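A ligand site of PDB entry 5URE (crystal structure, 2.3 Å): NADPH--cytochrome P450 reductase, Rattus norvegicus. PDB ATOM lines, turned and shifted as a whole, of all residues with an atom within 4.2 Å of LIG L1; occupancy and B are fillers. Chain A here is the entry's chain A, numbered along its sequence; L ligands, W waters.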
ATOM      1  N   TYR A  84      -4.212 -12.104  12.395  1.00  0.00           N
ATOM      2  CA  TYR A  84      -5.342 -11.740  13.241  1.00  0.00           C
ATOM      3  C   TYR A  84      -5.079 -10.417  13.929  1.00  0.00           C
ATOM      4  O   TYR A  84      -3.949  -9.926  13.939  1.00  0.00           O
ATOM      5  CB  TYR A  84      -5.637 -12.823  14.275  1.00  0.00           C
ATOM      6  CG  TYR A  84      -7.025 -12.694  14.882  1.00  0.00           C
ATOM      7  CD1 TYR A  84      -8.159 -12.775  14.078  1.00  0.00           C
ATOM      8  CD2 TYR A  84      -7.199 -12.477  16.248  1.00  0.00           C
ATOM      9  CE1 TYR A  84      -9.435 -12.627  14.614  1.00  0.00           C
ATOM     10  CE2 TYR A  84      -8.473 -12.330  16.802  1.00  0.00           C
ATOM     11  CZ  TYR A  84      -9.581 -12.405  15.966  1.00  0.00           C
ATOM     12  OH  TYR A  84     -10.852 -12.272  16.478  1.00  0.00           O
ATOM     13  N   HIS A 263     -13.479  -8.747  23.844  1.00  0.00           N
ATOM     14  CA  HIS A 263     -14.469  -9.507  23.106  1.00  0.00           C
ATOM     15  C   HIS A 263     -14.926 -10.666  23.969  1.00  0.00           C
ATOM     16  O   HIS A 263     -14.195 -11.114  24.841  1.00  0.00           O
ATOM     17  CB  HIS A 263     -13.862 -10.042  21.805  1.00  0.00           C
ATOM     18  CG  HIS A 263     -13.421  -8.963  20.853  1.00  0.00           C
ATOM     19  ND1 HIS A 263     -12.168  -8.944  20.273  1.00  0.00           N
ATOM     20  CD2 HIS A 263     -14.080  -7.881  20.366  1.00  0.00           C
ATOM     21  CE1 HIS A 263     -12.063  -7.891  19.485  1.00  0.00           C
ATOM     22  NE2 HIS A 263     -13.210  -7.228  19.516  1.00  0.00           N
ATOM     23  N   ARG A 368     -24.510 -19.571  -1.522  1.00  0.00           N
ATOM     24  CA  ARG A 368     -24.477 -19.862  -0.094  1.00  0.00           C
ATOM     25  C   ARG A 368     -25.223 -21.152   0.247  1.00  0.00           C
ATOM     26  O   ARG A 368     -26.076 -21.161   1.133  1.00  0.00           O
ATOM     27  CB  ARG A 368     -25.065 -18.701   0.715  1.00  0.00           C
ATOM     28  CG  ARG A 368     -24.339 -17.364   0.535  1.00  0.00           C
ATOM     29  CD  ARG A 368     -22.919 -17.419   1.069  1.00  0.00           C
ATOM     30  NE  ARG A 368     -22.891 -17.823   2.470  1.00  0.00           N
ATOM     31  CZ  ARG A 368     -21.781 -18.014   3.179  1.00  0.00           C
ATOM     32  NH1 ARG A 368     -21.854 -18.381   4.456  1.00  0.00           N
ATOM     33  NH2 ARG A 368     -20.589 -17.838   2.604  1.00  0.00           N
ATOM     34  N   ARG A 398     -18.280 -17.594  18.190  1.00  0.00           N
ATOM     35  CA  ARG A 398     -18.444 -16.303  17.541  1.00  0.00           C
ATOM     36  C   ARG A 398     -18.019 -15.250  18.559  1.00  0.00           C
ATOM     37  O   ARG A 398     -18.239 -15.421  19.751  1.00  0.00           O
ATOM     38  CB  ARG A 398     -19.907 -16.063  17.156  1.00  0.00           C
ATOM     39  CG  ARG A 398     -20.317 -16.552  15.788  1.00  0.00           C
ATOM     40  CD  ARG A 398     -20.217 -18.060  15.663  1.00  0.00           C
ATOM     41  NE  ARG A 398     -20.883 -18.498  14.438  1.00  0.00           N
ATOM     42  CZ  ARG A 398     -20.611 -19.638  13.810  1.00  0.00           C
ATOM     43  NH1 ARG A 398     -21.276 -19.958  12.700  1.00  0.00           N
ATOM     44  NH2 ARG A 398     -19.671 -20.450  14.263  1.00  0.00           N
ATOM     45  N   TYR A 399     -17.416 -14.161  18.083  1.00  0.00           N
ATOM     46  CA  TYR A 399     -16.984 -13.104  18.967  1.00  0.00           C
ATOM     47  C   TYR A 399     -17.974 -11.951  18.937  1.00  0.00           C
ATOM     48  O   TYR A 399     -18.622 -11.707  17.918  1.00  0.00           O
ATOM     49  CB  TYR A 399     -15.614 -12.562  18.556  1.00  0.00           C
ATOM     50  CG  TYR A 399     -14.512 -13.578  18.630  1.00  0.00           C
ATOM     51  CD1 TYR A 399     -13.927 -13.914  19.847  1.00  0.00           C
ATOM     52  CD2 TYR A 399     -14.060 -14.216  17.481  1.00  0.00           C
ATOM     53  CE1 TYR A 399     -12.905 -14.858  19.913  1.00  0.00           C
ATOM     54  CE2 TYR A 399     -13.044 -15.166  17.524  1.00  0.00           C
ATOM     55  CZ  TYR A 399     -12.477 -15.479  18.749  1.00  0.00           C
ATOM     56  OH  TYR A 399     -11.462 -16.407  18.804  1.00  0.00           O
ATOM     57  N   TYR A 400     -18.071 -11.244  20.050  1.00  0.00           N
ATOM     58  CA  TYR A 400     -18.941 -10.080  20.162  1.00  0.00           C
ATOM     59  C   TYR A 400     -18.207  -9.062  21.023  1.00  0.00           C
ATOM     60  O   TYR A 400     -17.596  -9.415  22.023  1.00  0.00           O
ATOM     61  CB  TYR A 400     -20.258 -10.507  20.783  1.00  0.00           C
ATOM     62  CG  TYR A 400     -21.050 -11.389  19.856  1.00  0.00           C
ATOM     63  CD1 TYR A 400     -21.814 -10.833  18.823  1.00  0.00           C
ATOM     64  CD2 TYR A 400     -20.966 -12.780  19.934  1.00  0.00           C
ATOM     65  CE1 TYR A 400     -22.478 -11.636  17.902  1.00  0.00           C
ATOM     66  CE2 TYR A 400     -21.631 -13.598  19.012  1.00  0.00           C
ATOM     67  CZ  TYR A 400     -22.371 -13.009  17.990  1.00  0.00           C
ATOM     68  OH  TYR A 400     -22.993 -13.787  17.038  1.00  0.00           O
ATOM     69  N   SER A 401     -18.236  -7.800  20.600  1.00  0.00           N
ATOM     70  CA  SER A 401     -17.558  -6.743  21.327  1.00  0.00           C
ATOM     71  C   SER A 401     -18.355  -6.413  22.576  1.00  0.00           C
ATOM     72  O   SER A 401     -19.440  -5.853  22.489  1.00  0.00           O
ATOM     73  CB  SER A 401     -17.397  -5.515  20.431  1.00  0.00           C
ATOM     74  OG  SER A 401     -16.742  -5.852  19.216  1.00  0.00           O
ATOM     75  N   CYS A 416     -24.208  -6.676  21.904  1.00  0.00           N
ATOM     76  CA  CYS A 416     -25.029  -5.932  20.958  1.00  0.00           C
ATOM     77  C   CYS A 416     -24.867  -6.575  19.587  1.00  0.00           C
ATOM     78  O   CYS A 416     -23.808  -6.455  18.968  1.00  0.00           O
ATOM     79  CB  CYS A 416     -24.601  -4.468  20.892  1.00  0.00           C
ATOM     80  SG  CYS A 416     -25.425  -3.540  19.565  1.00  0.00           S
ATOM     81  N   ALA A 417     -25.906  -7.245  19.094  1.00  0.00           N
ATOM     82  CA  ALA A 417     -25.806  -7.912  17.808  1.00  0.00           C
ATOM     83  C   ALA A 417     -27.046  -7.871  16.912  1.00  0.00           C
ATOM     84  O   ALA A 417     -28.181  -7.801  17.405  1.00  0.00           O
ATOM     85  CB  ALA A 417     -25.417  -9.362  18.022  1.00  0.00           C
ATOM     86  N   VAL A 418     -26.822  -7.932  15.606  1.00  0.00           N
ATOM     87  CA  VAL A 418     -27.925  -7.962  14.662  1.00  0.00           C
ATOM     88  C   VAL A 418     -28.086  -9.411  14.234  1.00  0.00           C
ATOM     89  O   VAL A 418     -27.098 -10.068  13.902  1.00  0.00           O
ATOM     90  CB  VAL A 418     -27.652  -7.068  13.403  1.00  0.00           C
ATOM     91  CG1 VAL A 418     -26.324  -7.432  12.761  1.00  0.00           C
ATOM     92  CG2 VAL A 418     -28.796  -7.241  12.392  1.00  0.00           C
ATOM     93  N   VAL A 420     -28.709 -12.523  11.972  1.00  0.00           N
ATOM     94  CA  VAL A 420     -28.467 -12.810  10.569  1.00  0.00           C
ATOM     95  C   VAL A 420     -29.568 -13.699  10.008  1.00  0.00           C
ATOM     96  O   VAL A 420     -29.862 -14.760  10.555  1.00  0.00           O
ATOM     97  CB  VAL A 420     -27.080 -13.493  10.374  1.00  0.00           C
ATOM     98  CG1 VAL A 420     -26.894 -13.887   8.931  1.00  0.00           C
ATOM     99  CG2 VAL A 420     -25.958 -12.546  10.815  1.00  0.00           C
ATOM    100  N   TYR A 422     -31.138 -14.067   5.846  1.00  0.00           N
ATOM    101  CA  TYR A 422     -31.253 -13.514   4.498  1.00  0.00           C
ATOM    102  C   TYR A 422     -31.704 -14.528   3.460  1.00  0.00           C
ATOM    103  O   TYR A 422     -31.638 -15.724   3.685  1.00  0.00           O
ATOM    104  CB  TYR A 422     -29.899 -12.955   4.065  1.00  0.00           C
ATOM    105  CG  TYR A 422     -28.789 -13.992   4.103  1.00  0.00           C
ATOM    106  CD1 TYR A 422     -28.172 -14.353   5.300  1.00  0.00           C
ATOM    107  CD2 TYR A 422     -28.403 -14.658   2.941  1.00  0.00           C
ATOM    108  CE1 TYR A 422     -27.179 -15.357   5.336  1.00  0.00           C
ATOM    109  CE2 TYR A 422     -27.423 -15.653   2.961  1.00  0.00           C
ATOM    110  CZ  TYR A 422     -26.825 -16.005   4.165  1.00  0.00           C
ATOM    111  OH  TYR A 422     -25.902 -17.028   4.165  1.00  0.00           O
ATOM    112  N   LYS A 431     -29.969 -18.831   8.066  1.00  0.00           N
ATOM    113  CA  LYS A 431     -29.978 -18.290   9.426  1.00  0.00           C
ATOM    114  C   LYS A 431     -28.595 -18.252  10.048  1.00  0.00           C
ATOM    115  O   LYS A 431     -27.820 -19.205   9.912  1.00  0.00           O
ATOM    116  CB  LYS A 431     -30.889 -19.139  10.324  1.00  0.00           C
ATOM    117  CG  LYS A 431     -32.340 -19.232   9.861  1.00  0.00           C
ATOM    118  CD  LYS A 431     -33.079 -17.915  10.068  1.00  0.00           C
ATOM    119  CE  LYS A 431     -34.224 -18.073  11.057  1.00  0.00           C
ATOM    120  NZ  LYS A 431     -33.779 -18.407  12.436  1.00  0.00           N
ATOM    121  N   GLY A 432     -28.267 -17.178  10.745  1.00  0.00           N
ATOM    122  CA  GLY A 432     -26.975 -17.087  11.393  1.00  0.00           C
ATOM    123  C   GLY A 432     -27.008 -18.026  12.586  1.00  0.00           C
ATOM    124  O   GLY A 432     -27.916 -17.954  13.399  1.00  0.00           O
ATOM    125  N   VAL A 433     -26.017 -18.910  12.686  1.00  0.00           N
ATOM    126  CA  VAL A 433     -25.977 -19.867  13.780  1.00  0.00           C
ATOM    127  C   VAL A 433     -26.041 -19.250  15.177  1.00  0.00           C
ATOM    128  O   VAL A 433     -26.991 -19.493  15.922  1.00  0.00           O
ATOM    129  CB  VAL A 433     -24.706 -20.777  13.718  1.00  0.00           C
ATOM    130  CG1 VAL A 433     -24.736 -21.798  14.844  1.00  0.00           C
ATOM    131  CG2 VAL A 433     -24.618 -21.476  12.374  1.00  0.00           C
ATOM    132  N   ALA A 434     -25.054 -18.428  15.530  1.00  0.00           N
ATOM    133  CA  ALA A 434     -25.010 -17.821  16.854  1.00  0.00           C
ATOM    134  C   ALA A 434     -26.096 -16.795  17.127  1.00  0.00           C
ATOM    135  O   ALA A 434     -26.660 -16.763  18.231  1.00  0.00           O
ATOM    136  CB  ALA A 434     -23.619 -17.202  17.117  1.00  0.00           C
ATOM    137  N   THR A 435     -26.402 -15.935  16.177  1.00  0.00           N
ATOM    138  CA  THR A 435     -27.430 -14.937  16.444  1.00  0.00           C
ATOM    139  C   THR A 435     -28.814 -15.575  16.551  1.00  0.00           C
ATOM    140  O   THR A 435     -29.610 -15.161  17.387  1.00  0.00           O
ATOM    141  CB  THR A 435     -27.414 -13.824  15.386  1.00  0.00           C
ATOM    142  OG1 THR A 435     -27.454 -14.404  14.080  1.00  0.00           O
ATOM    143  CG2 THR A 435     -26.140 -12.976  15.533  1.00  0.00           C
ATOM    144  N   THR A 479     -24.099  -1.661  14.436  1.00  0.00           N
ATOM    145  CA  THR A 479     -23.715  -2.458  15.598  1.00  0.00           C
ATOM    146  C   THR A 479     -22.276  -2.156  16.012  1.00  0.00           C
ATOM    147  O   THR A 479     -21.804  -2.609  17.059  1.00  0.00           O
ATOM    148  CB  THR A 479     -23.843  -3.979  15.309  1.00  0.00           C
ATOM    149  OG1 THR A 479     -22.921  -4.351  14.292  1.00  0.00           O
ATOM    150  CG2 THR A 479     -25.252  -4.304  14.840  1.00  0.00           C
ATOM    151  N   ALA A 482     -21.291  -1.117  19.642  1.00  0.00           N
ATOM    152  CA  ALA A 482     -21.150  -2.036  20.759  1.00  0.00           C
ATOM    153  C   ALA A 482     -20.075  -1.722  21.815  1.00  0.00           C
ATOM    154  O   ALA A 482     -20.410  -1.431  22.964  1.00  0.00           O
ATOM    155  CB  ALA A 482     -20.949  -3.457  20.229  1.00  0.00           C
ATOM    156  N   ASP A 619     -11.614  -2.111  15.666  1.00  0.00           N
ATOM    157  CA  ASP A 619     -12.340  -3.298  16.067  1.00  0.00           C
ATOM    158  C   ASP A 619     -13.272  -3.445  14.886  1.00  0.00           C
ATOM    159  O   ASP A 619     -14.458  -3.108  14.965  1.00  0.00           O
ATOM    160  CB  ASP A 619     -13.148  -3.096  17.347  1.00  0.00           C
ATOM    161  CG  ASP A 619     -13.848  -4.373  17.789  1.00  0.00           C
ATOM    162  OD1 ASP A 619     -13.416  -5.450  17.331  1.00  0.00           O
ATOM    163  OD2 ASP A 619     -14.801  -4.304  18.611  1.00  0.00           O
ATOM    164  N   TRP A 621     -14.891  -5.847  11.753  1.00  0.00           N
ATOM    165  CA  TRP A 621     -15.282  -7.228  11.496  1.00  0.00           C
ATOM    166  C   TRP A 621     -15.453  -7.669  10.065  1.00  0.00           C
ATOM    167  O   TRP A 621     -15.792  -6.886   9.178  1.00  0.00           O
ATOM    168  CB  TRP A 621     -16.556  -7.557  12.267  1.00  0.00           C
ATOM    169  CG  TRP A 621     -16.653  -6.842  13.584  1.00  0.00           C
ATOM    170  CD1 TRP A 621     -15.653  -6.672  14.501  1.00  0.00           C
ATOM    171  CD2 TRP A 621     -17.802  -6.195  14.130  1.00  0.00           C
ATOM    172  NE1 TRP A 621     -16.106  -5.953  15.577  1.00  0.00           N
ATOM    173  CE2 TRP A 621     -17.432  -5.649  15.382  1.00  0.00           C
ATOM    174  CE3 TRP A 621     -19.121  -6.026  13.691  1.00  0.00           C
ATOM    175  CZ2 TRP A 621     -18.324  -4.939  16.184  1.00  0.00           C
ATOM    176  CZ3 TRP A 621     -20.009  -5.324  14.499  1.00  0.00           C
ATOM    177  CH2 TRP A 621     -19.602  -4.794  15.718  1.00  0.00           C
HETATM  178  P1  LIG L   1     -23.051 -17.214  10.682  1.00  0.00           P
HETATM  179  O1  LIG L   1     -23.924 -18.407  10.642  1.00  0.00           O
HETATM  180  O2  LIG L   1     -21.700 -17.334  11.266  1.00  0.00           O
HETATM  181  O3  LIG L   1     -22.942 -16.623   9.191  1.00  0.00           O
HETATM  182  C1  LIG L   1     -22.069 -15.526   8.897  1.00  0.00           C
HETATM  183  C2  LIG L   1     -21.930 -15.407   7.379  1.00  0.00           C
HETATM  184  O4  LIG L   1     -23.207 -15.250   6.740  1.00  0.00           O
HETATM  185  C3  LIG L   1     -21.221 -14.126   6.995  1.00  0.00           C
HETATM  186  O5  LIG L   1     -19.806 -14.298   7.207  1.00  0.00           O
HETATM  187  C4  LIG L   1     -21.503 -14.155   5.503  1.00  0.00           C
HETATM  188  O6  LIG L   1     -20.640 -15.109   4.861  1.00  0.00           O
HETATM  189  C5  LIG L   1     -22.942 -14.654   5.452  1.00  0.00           C
HETATM  190  N1  LIG L   1     -23.906 -13.542   5.284  1.00  0.00           N
HETATM  191  C6  LIG L   1     -24.350 -12.603   6.334  1.00  0.00           C
HETATM  192  N2  LIG L   1     -25.372 -11.837   5.584  1.00  0.00           N
HETATM  193  C7  LIG L   1     -25.375 -12.251   4.322  1.00  0.00           C
HETATM  194  C8  LIG L   1     -26.129 -11.839   3.300  1.00  0.00           C
HETATM  195  N3  LIG L   1     -27.111 -10.990   3.604  1.00  0.00           N
HETATM  196  N4  LIG L   1     -25.990 -12.327   2.059  1.00  0.00           N
HETATM  197  C9  LIG L   1     -25.023 -13.305   1.826  1.00  0.00           C
HETATM  198  N5  LIG L   1     -24.243 -13.715   2.910  1.00  0.00           N
HETATM  199  C10 LIG L   1     -24.442 -13.184   4.122  1.00  0.00           C
HETATM  200  N6  LIG L   1     -21.281  -8.754  15.228  1.00  0.00           N
HETATM  201  C11 LIG L   1     -22.235  -8.020  15.937  1.00  0.00           C
HETATM  202  O7  LIG L   1     -23.416  -8.061  15.589  1.00  0.00           O
HETATM  203  N7  LIG L   1     -21.858  -7.329  17.089  1.00  0.00           N
HETATM  204  C12 LIG L   1     -20.543  -7.385  17.545  1.00  0.00           C
HETATM  205  O8  LIG L   1     -20.251  -6.874  18.627  1.00  0.00           O
HETATM  206  C13 LIG L   1     -19.596  -8.133  16.859  1.00  0.00           C
HETATM  207  N8  LIG L   1     -18.299  -8.047  17.170  1.00  0.00           N
HETATM  208  C14 LIG L   1     -17.400  -8.790  16.505  1.00  0.00           C
HETATM  209  C15 LIG L   1     -16.049  -8.732  16.853  1.00  0.00           C
HETATM  210  C16 LIG L   1     -15.122  -9.507  16.161  1.00  0.00           C
HETATM  211  C17 LIG L   1     -13.784  -9.499  16.560  1.00  0.00           C
HETATM  212  C18 LIG L   1     -15.533 -10.333  15.122  1.00  0.00           C
HETATM  213  C19 LIG L   1     -14.614 -11.107  14.437  1.00  0.00           C
HETATM  214  C20 LIG L   1     -16.888 -10.413  14.803  1.00  0.00           C
HETATM  215  C21 LIG L   1     -17.822  -9.674  15.505  1.00  0.00           C
HETATM  216  N9  LIG L   1     -19.130  -9.737  15.195  1.00  0.00           N
HETATM  217  C22 LIG L   1     -19.957  -8.811  15.694  1.00  0.00           C
HETATM  218  C23 LIG L   1     -19.638 -10.690  14.193  1.00  0.00           C
HETATM  219  C24 LIG L   1     -20.001 -11.990  14.915  1.00  0.00           C
HETATM  220  O9  LIG L   1     -18.819 -12.568  15.464  1.00  0.00           O
HETATM  221  C25 LIG L   1     -20.666 -13.014  13.997  1.00  0.00           C
HETATM  222  O10 LIG L   1     -19.841 -13.272  12.853  1.00  0.00           O
HETATM  223  C26 LIG L   1     -22.051 -12.539  13.558  1.00  0.00           C
HETATM  224  O11 LIG L   1     -22.863 -12.311  14.706  1.00  0.00           O
HETATM  225  C27 LIG L   1     -22.690 -13.616  12.677  1.00  0.00           C
HETATM  226  O12 LIG L   1     -22.710 -14.853  13.382  1.00  0.00           O
HETATM  227  P2  LIG L   1     -23.838 -15.961  13.075  1.00  0.00           P
HETATM  228  O13 LIG L   1     -25.147 -15.423  13.519  1.00  0.00           O
HETATM  229  O14 LIG L   1     -23.387 -17.265  13.632  1.00  0.00           O
HETATM  230  O15 LIG L   1     -23.843 -16.051  11.466  1.00  0.00           O
HETATM  231  P1  LG2 L   2     -26.181  -1.298   8.917  1.00  0.00           P
HETATM  232  O1  LG2 L   2     -27.523  -0.728   9.162  1.00  0.00           O
HETATM  233  O2  LG2 L   2     -26.017  -2.277   7.816  1.00  0.00           O
HETATM  234  O3  LG2 L   2     -25.128  -0.103   8.735  1.00  0.00           O
HETATM  235  C1  LG2 L   2     -25.053   0.902   9.760  1.00  0.00           C
HETATM  236  C2  LG2 L   2     -24.926   2.289   9.122  1.00  0.00           C
HETATM  237  O4  LG2 L   2     -23.726   2.350   8.333  1.00  0.00           O
HETATM  238  C3  LG2 L   2     -26.083   2.536   8.164  1.00  0.00           C
HETATM  239  O5  LG2 L   2     -26.534   3.896   8.322  1.00  0.00           O
HETATM  240  C4  LG2 L   2     -25.436   2.354   6.799  1.00  0.00           C
HETATM  241  O6  LG2 L   2     -26.136   3.136   5.822  1.00  0.00           O
HETATM  242  C5  LG2 L   2     -24.104   3.006   7.113  1.00  0.00           C
HETATM  243  N1  LG2 L   2     -23.070   2.815   6.072  1.00  0.00           N
HETATM  244  C6  LG2 L   2     -23.132   1.986   5.030  1.00  0.00           C
HETATM  245  N2  LG2 L   2     -21.973   2.053   4.395  1.00  0.00           N
HETATM  246  C7  LG2 L   2     -21.194   2.925   5.026  1.00  0.00           C
HETATM  247  C8  LG2 L   2     -19.966   3.371   4.766  1.00  0.00           C
HETATM  248  N3  LG2 L   2     -19.460   3.042   3.574  1.00  0.00           N
HETATM  249  N4  LG2 L   2     -19.358   4.263   5.550  1.00  0.00           N
HETATM  250  C9  LG2 L   2     -20.013   4.730   6.690  1.00  0.00           C
HETATM  251  N5  LG2 L   2     -21.309   4.242   6.936  1.00  0.00           N
HETATM  252  C10 LG2 L   2     -21.867   3.368   6.085  1.00  0.00           C
HETATM  253  O7  LG2 L   2     -25.677  -1.993  10.276  1.00  0.00           O
HETATM  254  P2  LG2 L   2     -24.878  -3.330  10.690  1.00  0.00           P
HETATM  255  O8  LG2 L   2     -25.812  -4.474  10.651  1.00  0.00           O
HETATM  256  O9  LG2 L   2     -24.141  -3.050  11.938  1.00  0.00           O
HETATM  257  O10 LG2 L   2     -23.844  -3.508   9.476  1.00  0.00           O
HETATM  258  C11 LG2 L   2     -23.043  -2.406   9.031  1.00  0.00           C
HETATM  259  C12 LG2 L   2     -21.942  -2.906   8.100  1.00  0.00           C
HETATM  260  O11 LG2 L   2     -21.116  -3.829   8.835  1.00  0.00           O
HETATM  261  C13 LG2 L   2     -22.541  -3.709   6.960  1.00  0.00           C
HETATM  262  O12 LG2 L   2     -21.706  -3.626   5.794  1.00  0.00           O
HETATM  263  C14 LG2 L   2     -22.492  -5.120   7.514  1.00  0.00           C
HETATM  264  O13 LG2 L   2     -22.531  -6.071   6.447  1.00  0.00           O
HETATM  265  C15 LG2 L   2     -21.085  -5.054   8.083  1.00  0.00           C
HETATM  266  N6  LG2 L   2     -20.726  -6.221   8.908  1.00  0.00           N
HETATM  267  C16 LG2 L   2     -21.424  -6.504  10.084  1.00  0.00           C
HETATM  268  C17 LG2 L   2     -21.138  -7.661  10.805  1.00  0.00           C
HETATM  269  C18 LG2 L   2     -21.824  -7.917  11.993  1.00  0.00           C
HETATM  270  O14 LG2 L   2     -22.309  -6.990  12.652  1.00  0.00           O
HETATM  271  N7  LG2 L   2     -21.738  -9.164  12.435  1.00  0.00           N
HETATM  272  C19 LG2 L   2     -20.166  -8.540  10.349  1.00  0.00           C
HETATM  273  C20 LG2 L   2     -19.450  -8.259   9.194  1.00  0.00           C
HETATM  274  C21 LG2 L   2     -19.725  -7.111   8.473  1.00  0.00           C
HETATM  275  P3  LG2 L   2     -26.918   2.455   4.591  1.00  0.00           P
HETATM  276  O15 LG2 L   2     -27.123   1.041   5.013  1.00  0.00           O
HETATM  277  O16 LG2 L   2     -26.001   2.614   3.439  1.00  0.00           O
HETATM  278  O17 LG2 L   2     -28.169   3.246   4.501  1.00  0.00           O
HETATM  279  N1  LG3 L   3      -6.225 -10.475   7.541  1.00  0.00           N
HETATM  280  C1  LG3 L   3      -5.092  -9.804   7.239  1.00  0.00           C
HETATM  281  O1  LG3 L   3      -4.492  -9.997   6.178  1.00  0.00           O
HETATM  282  N2  LG3 L   3      -4.646  -8.892   8.187  1.00  0.00           N
HETATM  283  C2  LG3 L   3      -5.234  -8.584   9.408  1.00  0.00           C
HETATM  284  O2  LG3 L   3      -4.648  -7.743  10.075  1.00  0.00           O
HETATM  285  C3  LG3 L   3      -6.426  -9.278   9.718  1.00  0.00           C
HETATM  286  N3  LG3 L   3      -7.058  -8.972  10.949  1.00  0.00           N
HETATM  287  C4  LG3 L   3      -8.259  -9.661  11.156  1.00  0.00           C
HETATM  288  C5  LG3 L   3      -8.958  -9.327  12.380  1.00  0.00           C
HETATM  289  C6  LG3 L   3     -10.198  -9.930  12.704  1.00  0.00           C
HETATM  290  C7  LG3 L   3     -10.827  -9.464  14.033  1.00  0.00           C
HETATM  291  C8  LG3 L   3     -10.821 -10.944  11.789  1.00  0.00           C
HETATM  292  C9  LG3 L   3     -12.023 -11.597  11.975  1.00  0.00           C
HETATM  293  C10 LG3 L   3     -10.153 -11.270  10.619  1.00  0.00           C
HETATM  294  C11 LG3 L   3      -8.866 -10.656  10.258  1.00  0.00           C
HETATM  295  N4  LG3 L   3      -8.120 -10.938   9.020  1.00  0.00           N
HETATM  296  C12 LG3 L   3      -6.866 -10.224   8.734  1.00  0.00           C
HETATM  297  C13 LG3 L   3      -8.624 -11.914   8.057  1.00  0.00           C
HETATM  298  C14 LG3 L   3      -8.188 -13.386   8.377  1.00  0.00           C
HETATM  299  O3  LG3 L   3      -6.706 -13.459   8.361  1.00  0.00           O
HETATM  300  C15 LG3 L   3      -8.749 -14.346   7.343  1.00  0.00           C
HETATM  301  O4  LG3 L   3     -10.185 -14.245   7.426  1.00  0.00           O
HETATM  302  C16 LG3 L   3      -8.245 -15.792   7.711  1.00  0.00           C
HETATM  303  O5  LG3 L   3      -8.828 -16.586   6.651  1.00  0.00           O
HETATM  304  C17 LG3 L   3      -8.808 -16.364   9.000  1.00  0.00           C
HETATM  305  O6  LG3 L   3      -8.238 -17.693   9.263  1.00  0.00           O
HETATM  306  P1  LG3 L   3      -8.553 -18.658  10.465  1.00  0.00           P
HETATM  307  O7  LG3 L   3      -9.956 -19.123  10.360  1.00  0.00           O
HETATM  308  O8  LG3 L   3      -8.092 -17.844  11.720  1.00  0.00           O
HETATM  309  O9  LG3 L   3      -7.542 -19.812  10.036  1.00  0.00           O
HETATM  310  O   HOH W   1     -16.712 -14.442  15.168  1.00  0.00           O
HETATM  311  O   HOH W   2     -24.718 -17.486   6.520  1.00  0.00           O
HETATM  312  O   HOH W   3     -19.577 -15.935  12.252  1.00  0.00           O
HETATM  313  O   HOH W   4     -25.694 -19.263   8.400  1.00  0.00           O
HETATM  314  O   HOH W   5     -24.431 -10.334  13.981  1.00  0.00           O
HETATM  315  O   HOH W   6     -21.543  -6.923  21.150  1.00  0.00           O
HETATM  316  O   HOH W   7     -19.626 -18.346   9.923  1.00  0.00           O
HETATM  317  O   HOH W   8     -22.760 -20.150   8.967  1.00  0.00           O
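A nitrogen (N6) of LIG L1 is in hydrogen-bond range of a nitrogen (N7) of LG2 L2, at 2.9 Å.
Residues that only touch LIG L1: Gly 432 (3.3 Å), Ala 417 (3.3 Å), Tyr 422 (3.4 Å), Arg 368 (3.5 Å), His 263 (3.8 Å), Ala 482 (3.8 Å), Val 420 (3.9 Å) and Thr 479 (3.96 Å).
Hydrophobic or aromatic side chains within 4 Å of LIG L1: His 263, Tyr 399, Tyr 400, Ala 417, Val 420, Tyr 422, Val 433, Ala 434, Ala 482 and Trp 621.
Along chain A the residues within 4 Å of LIG L1 span positions 263 to 621.
The nearest printed residue that does not touch LIG L1 is Tyr 84 (4.04 Å).
Water W5 lies within hydrogen-bond range of O11 of LIG L1 (2.6 Å), O of Val 418 (2.7 Å) and N7 of LG2 L2 (3.3 Å).
Water W2 lies within hydrogen-bond range of the side-chain hydroxyl of Tyr 422 (2.7 Å) and an oxygen (O4) of LIG L1 (2.7 Å).
Water W6 lies within hydrogen-bond range of the backbone carbonyl oxygen of Ser 401 (2.7 Å), the backbone NH of Cys 416 (2.8 Å) and an oxygen (O8) of LIG L1 (2.8 Å).
Water W1 lies within hydrogen-bond range of an oxygen (O9) of LIG L1 and the backbone NH (N) of Tyr 399.
Water W4 bridges O of Lys 431 (2.6 Å) and O1 of LIG L1 (3.0 Å).
The backbone NH of Val 420 lies within hydrogen-bond range of the side-chain hydroxyl of Thr 435, 3.1 Å away.
The side-chain hydroxyl (OG) of Ser 401 lies within hydrogen-bond range of the side-chain carboxylate (OD2) of Asp 619 (2.6 Å).
NE1 of Trp 621 is in hydrogen-bond range of OD1 of Asp 619.
O of Val 420 is in hydrogen-bond range of N of Gly 432 (2.9 Å).
OD1 of Asp 619 sits at hydrogen-bond distance from NE2 of His 263.
N of Thr 435 is in hydrogen-bond range of O13 of LIG L1, at 3.0 Å.
The side-chain hydroxyl (OG1) of Thr 435 lies within hydrogen-bond range of an oxygen (O13) of LIG L1.
N of Tyr 399 sits at hydrogen-bond distance from O9 of LIG L1, 3.4 Å away.
O9 of LIG L1 is in hydrogen-bond range of O of Tyr 399 (2.6 Å).
The side-chain hydroxyl (OH) of Tyr 400 lies within hydrogen-bond range of an oxygen (O11) of LIG L1, at 2.8 Å.
N of Ala 434 sits at hydrogen-bond distance from O14 of LIG L1.
A nitrogen (N7) of LIG L1 lies within hydrogen-bond range of the backbone carbonyl oxygen of Cys 416, at 2.8 Å.
The guanidinium group of Arg 398 is in salt-bridge range of an oxygen (O14) of LIG L1 (2.9 Å).
O1 of LIG L1 lies within hydrogen-bond range of N of Val 433 (3.0 Å).
The backbone NH (N) of Ser 401 sits at hydrogen-bond distance from an oxygen (O8) of LIG L1 (3.0 Å).
OG of Ser 401 sits at hydrogen-bond distance from N8 of LIG L1.
The indole nitrogen of Trp 621 lies close to a nitrogen (N8) of LIG L1, at 3.4 Å.
An oxygen (O7) of LIG L1 sits at hydrogen-bond distance from the backbone NH of Val 418, 3.4 Å away.
The backbone NH (N) of Thr 479 sits at hydrogen-bond distance from an oxygen (O9) of LG2 L2 (2.9 Å).
The side-chain hydroxyl of Thr 479 is in hydrogen-bond range of an oxygen (O9) of LG2 L2 (3.0 Å).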
